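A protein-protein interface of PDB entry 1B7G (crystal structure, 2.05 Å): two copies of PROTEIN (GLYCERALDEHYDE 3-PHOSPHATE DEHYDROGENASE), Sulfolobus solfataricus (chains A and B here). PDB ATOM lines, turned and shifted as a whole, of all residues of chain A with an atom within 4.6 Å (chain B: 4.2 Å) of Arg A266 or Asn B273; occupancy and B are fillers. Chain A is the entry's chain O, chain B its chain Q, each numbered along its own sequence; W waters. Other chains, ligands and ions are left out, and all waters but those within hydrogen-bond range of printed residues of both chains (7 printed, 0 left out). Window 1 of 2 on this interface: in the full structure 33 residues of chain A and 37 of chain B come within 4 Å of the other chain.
NH2 of Arg B15 lies close to NH2 of Arg A266, at 3.2 Å.
NE of Arg B272 is in salt-bridge range of OD1 of Asp A267 (3.0 Å).
The side-chain carboxylate (OE1) of Glu B301 lies within salt-bridge range of the guanidinium group (NH2) of Arg A266, at 2.8 Å.
The side-chain carboxylate of Asp B274 lies within salt-bridge range of the guanidinium group of Arg A266 (3.8 Å).
NZ of Lys A269 is in salt-bridge range of OD2 of Asp B271, 2.7 Å away.
The guanidinium group (NH2) of Arg A266 is in hydrogen-bond range of the backbone carbonyl oxygen (O) of Arg B272 (2.7 Å).
The side-chain amide oxygen (OD1) of Asn A273 sits at hydrogen-bond distance from the guanidinium group (NE) of Arg B266 (3.4 Å).
ND2 of Asn A273 sits at hydrogen-bond distance from OD1 of Asn B273.
Arg A266 touches Asn B273, and with the chains exchanged Asn A273 touches Arg B266.
Asn B273 touches its own counterpart, Asn A273.
3 positions are printed for both chains.
Arg A266 touches five residues of chain B.
Asn B273 touches just these residues of chain A: Arg A266 and Asn A273.
Of the printed residues of chain A, Glu B301 touches Arg A266.
Printed residues of chain B within 4 Å of Asp A267: Arg B272 (3.0 Å).
Val A262 touches none of the printed residues of chain B.
The nearest printed residue of chain A that does not touch Asn B273 is Val A262 (6.4 Å).
The nearest printed residue of chain B that does not touch Asn A273 is Arg B272 (4.9 Å).
The guanidinium group (NH1) of Arg A266 lies within salt-bridge range of the side-chain carboxylate (OE1) of Glu A263, at 3.0 Å.
The side-chain carboxylate of Asp B274 lies within salt-bridge range of the guanidinium group of Arg B15 (2.7 Å).
NH2 of Arg B15 is in salt-bridge range of OE2 of Glu B301 (3.7 Å).
OD1 of Asp B271 is in salt-bridge range of NH1 of Arg B272, at 3.2 Å.
Among the printed residues, pairs that only touch across the chains: Arg A266 with Asn B273 (3.7 Å) and Lys A269 with Arg B272 (3.7 Å).
Of the 10 printed residues of chain B, 7 touch a printed residue of chain A.
Along chain B the printed residues that touch a printed residue of chain A span positions 15 to 301.
Among the printed residues, 10 pairs touch across the chains.
Water W7 lies within hydrogen-bond range of the side-chain carboxylate (OE2) of Glu A263 (2.6 Å), the guanidinium group (NH1) of Arg B15 (3.0 Å) and the side-chain carboxylate (OE2) of Glu B301 (3.1 Å).
Water W1 lies within hydrogen-bond range of the side-chain carboxylate (OE1) of Glu B301 (2.7 Å) and the guanidinium group (NH1) of Arg A266 (3.4 Å).
Water W5 bridges O of Arg A266 (2.7 Å) and N of Arg B272 (2.9 Å).
Water W6 lies within hydrogen-bond range of OE2 of Glu B301 (2.9 Å), OE1 of Glu A263 (2.9 Å) and NH1 of Arg A266 (3.4 Å).
Water W3 lies within hydrogen-bond range of NZ of Lys A269 and OD2 of Asp B271.
Water W2 lies within hydrogen-bond range of the side-chain carboxylate of Glu A263 (3.1 Å), the side-chain carboxylate of Asp A267 (3.1 Å) and the guanidinium group of Arg B15 (3.2 Å).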
ATOM      1  N   VAL A 262      26.742  -8.888  25.070  1.00  0.00           N
ATOM      2  CA  VAL A 262      26.600  -9.134  23.612  1.00  0.00           C
ATOM      3  C   VAL A 262      25.268  -8.526  23.165  1.00  0.00           C
ATOM      4  O   VAL A 262      25.156  -7.854  22.158  1.00  0.00           O
ATOM      5  CB  VAL A 262      26.644 -10.604  23.229  1.00  0.00           C
ATOM      6  CG1 VAL A 262      26.297 -10.897  21.741  1.00  0.00           C
ATOM      7  CG2 VAL A 262      28.033 -11.184  23.485  1.00  0.00           C
ATOM      8  N   GLU A 263      24.222  -8.750  23.952  1.00  0.00           N
ATOM      9  CA  GLU A 263      22.941  -8.170  23.705  1.00  0.00           C
ATOM     10  C   GLU A 263      22.992  -6.640  23.632  1.00  0.00           C
ATOM     11  O   GLU A 263      22.383  -6.091  22.723  1.00  0.00           O
ATOM     12  CB  GLU A 263      21.879  -8.574  24.745  1.00  0.00           C
ATOM     13  CG  GLU A 263      20.471  -8.403  24.188  1.00  0.00           C
ATOM     14  CD  GLU A 263      19.975  -9.413  23.209  1.00  0.00           C
ATOM     15  OE1 GLU A 263      20.668 -10.345  22.747  1.00  0.00           O
ATOM     16  OE2 GLU A 263      18.793  -9.271  22.796  1.00  0.00           O
ATOM     17  N   VAL A 264      23.618  -5.975  24.581  1.00  0.00           N
ATOM     18  CA  VAL A 264      23.756  -4.518  24.543  1.00  0.00           C
ATOM     19  C   VAL A 264      24.305  -4.063  23.190  1.00  0.00           C
ATOM     20  O   VAL A 264      23.797  -3.108  22.594  1.00  0.00           O
ATOM     21  CB  VAL A 264      24.663  -3.995  25.667  1.00  0.00           C
ATOM     22  CG1 VAL A 264      25.092  -2.536  25.412  1.00  0.00           C
ATOM     23  CG2 VAL A 264      23.928  -4.113  27.003  1.00  0.00           C
ATOM     24  N   ALA A 265      25.323  -4.761  22.702  1.00  0.00           N
ATOM     25  CA  ALA A 265      25.951  -4.429  21.444  1.00  0.00           C
ATOM     26  C   ALA A 265      25.019  -4.594  20.246  1.00  0.00           C
ATOM     27  O   ALA A 265      25.124  -3.797  19.278  1.00  0.00           O
ATOM     28  CB  ALA A 265      27.204  -5.271  21.232  1.00  0.00           C
ATOM     29  N   ARG A 266      24.233  -5.667  20.243  1.00  0.00           N
ATOM     30  CA  ARG A 266      23.237  -5.927  19.245  1.00  0.00           C
ATOM     31  C   ARG A 266      22.229  -4.760  19.215  1.00  0.00           C
ATOM     32  O   ARG A 266      21.986  -4.241  18.137  1.00  0.00           O
ATOM     33  CB  ARG A 266      22.452  -7.239  19.481  1.00  0.00           C
ATOM     34  CG  ARG A 266      23.280  -8.491  19.230  1.00  0.00           C
ATOM     35  CD  ARG A 266      22.495  -9.735  19.689  1.00  0.00           C
ATOM     36  NE  ARG A 266      21.700 -10.271  18.571  1.00  0.00           N
ATOM     37  CZ  ARG A 266      20.686 -11.121  18.757  1.00  0.00           C
ATOM     38  NH1 ARG A 266      20.304 -11.533  19.965  1.00  0.00           N
ATOM     39  NH2 ARG A 266      20.038 -11.553  17.692  1.00  0.00           N
ATOM     40  N   ASP A 267      21.672  -4.357  20.332  1.00  0.00           N
ATOM     41  CA  ASP A 267      20.700  -3.301  20.414  1.00  0.00           C
ATOM     42  C   ASP A 267      21.266  -1.902  20.163  1.00  0.00           C
ATOM     43  O   ASP A 267      20.496  -1.027  19.744  1.00  0.00           O
ATOM     44  CB  ASP A 267      19.998  -3.264  21.791  1.00  0.00           C
ATOM     45  CG  ASP A 267      19.093  -4.514  21.930  1.00  0.00           C
ATOM     46  OD1 ASP A 267      18.954  -5.235  20.927  1.00  0.00           O
ATOM     47  OD2 ASP A 267      18.563  -4.728  23.025  1.00  0.00           O
ATOM     48  N   LEU A 268      22.552  -1.705  20.390  1.00  0.00           N
ATOM     49  CA  LEU A 268      23.236  -0.457  20.089  1.00  0.00           C
ATOM     50  C   LEU A 268      23.608  -0.429  18.607  1.00  0.00           C
ATOM     51  O   LEU A 268      24.107   0.591  18.090  1.00  0.00           O
ATOM     52  CB  LEU A 268      24.507  -0.248  20.947  1.00  0.00           C
ATOM     53  CG  LEU A 268      24.284   0.202  22.390  1.00  0.00           C
ATOM     54  CD1 LEU A 268      25.629   0.222  23.136  1.00  0.00           C
ATOM     55  CD2 LEU A 268      23.659   1.585  22.493  1.00  0.00           C
ATOM     56  N   LYS A 269      23.394  -1.547  17.912  1.00  0.00           N
ATOM     57  CA  LYS A 269      23.639  -1.706  16.498  1.00  0.00           C
ATOM     58  C   LYS A 269      25.108  -1.550  16.150  1.00  0.00           C
ATOM     59  O   LYS A 269      25.497  -1.013  15.113  1.00  0.00           O
ATOM     60  CB  LYS A 269      22.729  -0.746  15.696  1.00  0.00           C
ATOM     61  CG  LYS A 269      21.250  -0.713  16.051  1.00  0.00           C
ATOM     62  CD  LYS A 269      20.552  -2.061  16.041  1.00  0.00           C
ATOM     63  CE  LYS A 269      19.085  -1.951  16.478  1.00  0.00           C
ATOM     64  NZ  LYS A 269      18.170  -1.506  15.375  1.00  0.00           N
ATOM     65  N   ASN A 273      28.050  -6.871  16.268  1.00  0.00           N
ATOM     66  CA  ASN A 273      27.912  -6.920  17.693  1.00  0.00           C
ATOM     67  C   ASN A 273      29.299  -6.821  18.362  1.00  0.00           C
ATOM     68  O   ASN A 273      29.367  -7.191  19.536  1.00  0.00           O
ATOM     69  CB  ASN A 273      27.216  -8.174  18.257  1.00  0.00           C
ATOM     70  CG  ASN A 273      26.304  -8.916  17.344  1.00  0.00           C
ATOM     71  OD1 ASN A 273      26.387 -10.148  17.213  1.00  0.00           O
ATOM     72  ND2 ASN A 273      25.481  -8.189  16.580  1.00  0.00           N
ATOM     73  N   ARG B  15      11.991  -5.637  18.385  1.00  0.00           N
ATOM     74  CA  ARG B  15      12.099  -5.790  16.941  1.00  0.00           C
ATOM     75  C   ARG B  15      10.886  -5.228  16.192  1.00  0.00           C
ATOM     76  O   ARG B  15      11.001  -4.501  15.192  1.00  0.00           O
ATOM     77  CB  ARG B  15      12.434  -7.213  16.533  1.00  0.00           C
ATOM     78  CG  ARG B  15      13.852  -7.664  16.968  1.00  0.00           C
ATOM     79  CD  ARG B  15      13.917  -9.220  16.847  1.00  0.00           C
ATOM     80  NE  ARG B  15      15.321  -9.639  16.889  1.00  0.00           N
ATOM     81  CZ  ARG B  15      16.015  -9.654  18.059  1.00  0.00           C
ATOM     82  NH1 ARG B  15      15.418  -9.361  19.198  1.00  0.00           N
ATOM     83  NH2 ARG B  15      17.285 -10.032  18.028  1.00  0.00           N
ATOM     84  N   ALA B 265      24.638 -13.930   8.867  1.00  0.00           N
ATOM     85  CA  ALA B 265      23.889 -12.745   9.172  1.00  0.00           C
ATOM     86  C   ALA B 265      24.708 -11.614   9.770  1.00  0.00           C
ATOM     87  O   ALA B 265      24.259 -10.458   9.621  1.00  0.00           O
ATOM     88  CB  ALA B 265      22.683 -13.021  10.027  1.00  0.00           C
ATOM     89  N   ARG B 266      25.782 -11.895  10.512  1.00  0.00           N
ATOM     90  CA  ARG B 266      26.611 -10.862  11.115  1.00  0.00           C
ATOM     91  C   ARG B 266      27.448 -10.161  10.040  1.00  0.00           C
ATOM     92  O   ARG B 266      27.530  -8.941   9.989  1.00  0.00           O
ATOM     93  CB  ARG B 266      27.567 -11.431  12.176  1.00  0.00           C
ATOM     94  CG  ARG B 266      26.833 -11.786  13.482  1.00  0.00           C
ATOM     95  CD  ARG B 266      27.830 -12.590  14.370  1.00  0.00           C
ATOM     96  NE  ARG B 266      28.646 -11.666  15.166  1.00  0.00           N
ATOM     97  CZ  ARG B 266      29.780 -12.001  15.779  1.00  0.00           C
ATOM     98  NH1 ARG B 266      30.277 -13.238  15.675  1.00  0.00           N
ATOM     99  NH2 ARG B 266      30.431 -11.095  16.503  1.00  0.00           N
ATOM    100  N   ARG B 270      23.043  -7.846   8.893  1.00  0.00           N
ATOM    101  CA  ARG B 270      21.581  -7.717   9.066  1.00  0.00           C
ATOM    102  C   ARG B 270      21.365  -7.148  10.465  1.00  0.00           C
ATOM    103  O   ARG B 270      22.193  -7.390  11.350  1.00  0.00           O
ATOM    104  CB  ARG B 270      20.875  -9.040   8.846  1.00  0.00           C
ATOM    105  CG  ARG B 270      21.348  -9.857   7.656  1.00  0.00           C
ATOM    106  CD  ARG B 270      20.358 -10.946   7.277  1.00  0.00           C
ATOM    107  NE  ARG B 270      19.089 -10.455   6.788  1.00  0.00           N
ATOM    108  CZ  ARG B 270      18.018 -11.178   6.486  1.00  0.00           C
ATOM    109  NH1 ARG B 270      18.014 -12.501   6.635  1.00  0.00           N
ATOM    110  NH2 ARG B 270      16.907 -10.580   6.061  1.00  0.00           N
ATOM    111  N   ASP B 271      20.371  -6.295  10.674  1.00  0.00           N
ATOM    112  CA  ASP B 271      20.082  -5.727  11.959  1.00  0.00           C
ATOM    113  C   ASP B 271      19.874  -6.831  13.012  1.00  0.00           C
ATOM    114  O   ASP B 271      19.118  -7.798  12.831  1.00  0.00           O
ATOM    115  CB  ASP B 271      18.821  -4.879  11.890  1.00  0.00           C
ATOM    116  CG  ASP B 271      18.535  -4.037  13.102  1.00  0.00           C
ATOM    117  OD1 ASP B 271      18.125  -4.585  14.133  1.00  0.00           O
ATOM    118  OD2 ASP B 271      18.716  -2.799  13.070  1.00  0.00           O
ATOM    119  N   ARG B 272      20.605  -6.665  14.122  1.00  0.00           N
ATOM    120  CA  ARG B 272      20.619  -7.579  15.231  1.00  0.00           C
ATOM    121  C   ARG B 272      20.986  -9.000  14.843  1.00  0.00           C
ATOM    122  O   ARG B 272      20.786  -9.918  15.640  1.00  0.00           O
ATOM    123  CB  ARG B 272      19.255  -7.611  15.941  1.00  0.00           C
ATOM    124  CG  ARG B 272      18.962  -6.356  16.740  1.00  0.00           C
ATOM    125  CD  ARG B 272      17.748  -6.507  17.615  1.00  0.00           C
ATOM    126  NE  ARG B 272      17.416  -5.301  18.389  1.00  0.00           N
ATOM    127  CZ  ARG B 272      16.664  -4.301  17.915  1.00  0.00           C
ATOM    128  NH1 ARG B 272      16.170  -4.306  16.688  1.00  0.00           N
ATOM    129  NH2 ARG B 272      16.413  -3.284  18.705  1.00  0.00           N
ATOM    130  N   ASN B 273      21.573  -9.252  13.693  1.00  0.00           N
ATOM    131  CA  ASN B 273      21.886 -10.478  13.045  1.00  0.00           C
ATOM    132  C   ASN B 273      20.620 -11.363  12.881  1.00  0.00           C
ATOM    133  O   ASN B 273      20.722 -12.584  12.868  1.00  0.00           O
ATOM    134  CB  ASN B 273      22.997 -11.320  13.613  1.00  0.00           C
ATOM    135  CG  ASN B 273      23.940 -10.659  14.588  1.00  0.00           C
ATOM    136  OD1 ASN B 273      24.626  -9.670  14.286  1.00  0.00           O
ATOM    137  ND2 ASN B 273      23.937 -11.191  15.817  1.00  0.00           N
ATOM    138  N   ASP B 274      19.469 -10.747  12.683  1.00  0.00           N
ATOM    139  CA  ASP B 274      18.222 -11.474  12.481  1.00  0.00           C
ATOM    140  C   ASP B 274      18.087 -12.141  11.127  1.00  0.00           C
ATOM    141  O   ASP B 274      18.546 -11.638  10.109  1.00  0.00           O
ATOM    142  CB  ASP B 274      17.056 -10.472  12.640  1.00  0.00           C
ATOM    143  CG  ASP B 274      16.906 -10.078  14.097  1.00  0.00           C
ATOM    144  OD1 ASP B 274      17.615 -10.721  14.922  1.00  0.00           O
ATOM    145  OD2 ASP B 274      16.141  -9.157  14.406  1.00  0.00           O
ATOM    146  N   ILE B 275      17.462 -13.318  11.078  1.00  0.00           N
ATOM    147  CA  ILE B 275      17.100 -13.982   9.808  1.00  0.00           C
ATOM    148  C   ILE B 275      15.629 -14.377   9.970  1.00  0.00           C
ATOM    149  O   ILE B 275      15.333 -15.418  10.549  1.00  0.00           O
ATOM    150  CB  ILE B 275      17.929 -15.194   9.463  1.00  0.00           C
ATOM    151  CG1 ILE B 275      19.426 -14.838   9.442  1.00  0.00           C
ATOM    152  CG2 ILE B 275      17.576 -15.900   8.139  1.00  0.00           C
ATOM    153  CD1 ILE B 275      20.334 -16.031   9.528  1.00  0.00           C
ATOM    154  N   GLU B 301      14.021 -15.246  17.324  1.00  0.00           N
ATOM    155  CA  GLU B 301      13.953 -13.853  17.749  1.00  0.00           C
ATOM    156  C   GLU B 301      13.241 -12.969  16.719  1.00  0.00           C
ATOM    157  O   GLU B 301      12.629 -11.968  17.116  1.00  0.00           O
ATOM    158  CB  GLU B 301      15.389 -13.292  17.965  1.00  0.00           C
ATOM    159  CG  GLU B 301      16.173 -14.099  19.016  1.00  0.00           C
ATOM    160  CD  GLU B 301      17.565 -13.531  19.289  1.00  0.00           C
ATOM    161  OE1 GLU B 301      18.463 -13.739  18.451  1.00  0.00           O
ATOM    162  OE2 GLU B 301      17.725 -12.937  20.350  1.00  0.00           O
HETATM  163  O   HOH W   1      20.883 -14.749  18.989  1.00  0.00           O
HETATM  164  O   HOH W   2      19.050  -8.156  19.944  1.00  0.00           O
HETATM  165  O   HOH W   3      16.307  -0.813  13.101  1.00  0.00           O
HETATM  166  O   HOH W   4      27.813 -11.977  18.529  1.00  0.00           O
HETATM  167  O   HOH W   5      22.447  -4.969  15.557  1.00  0.00           O
HETATM  168  O   HOH W   6      19.156 -12.859  22.883  1.00  0.00           O
HETATM  169  O   HOH W   7      16.652 -10.400  21.739  1.00  0.00           O
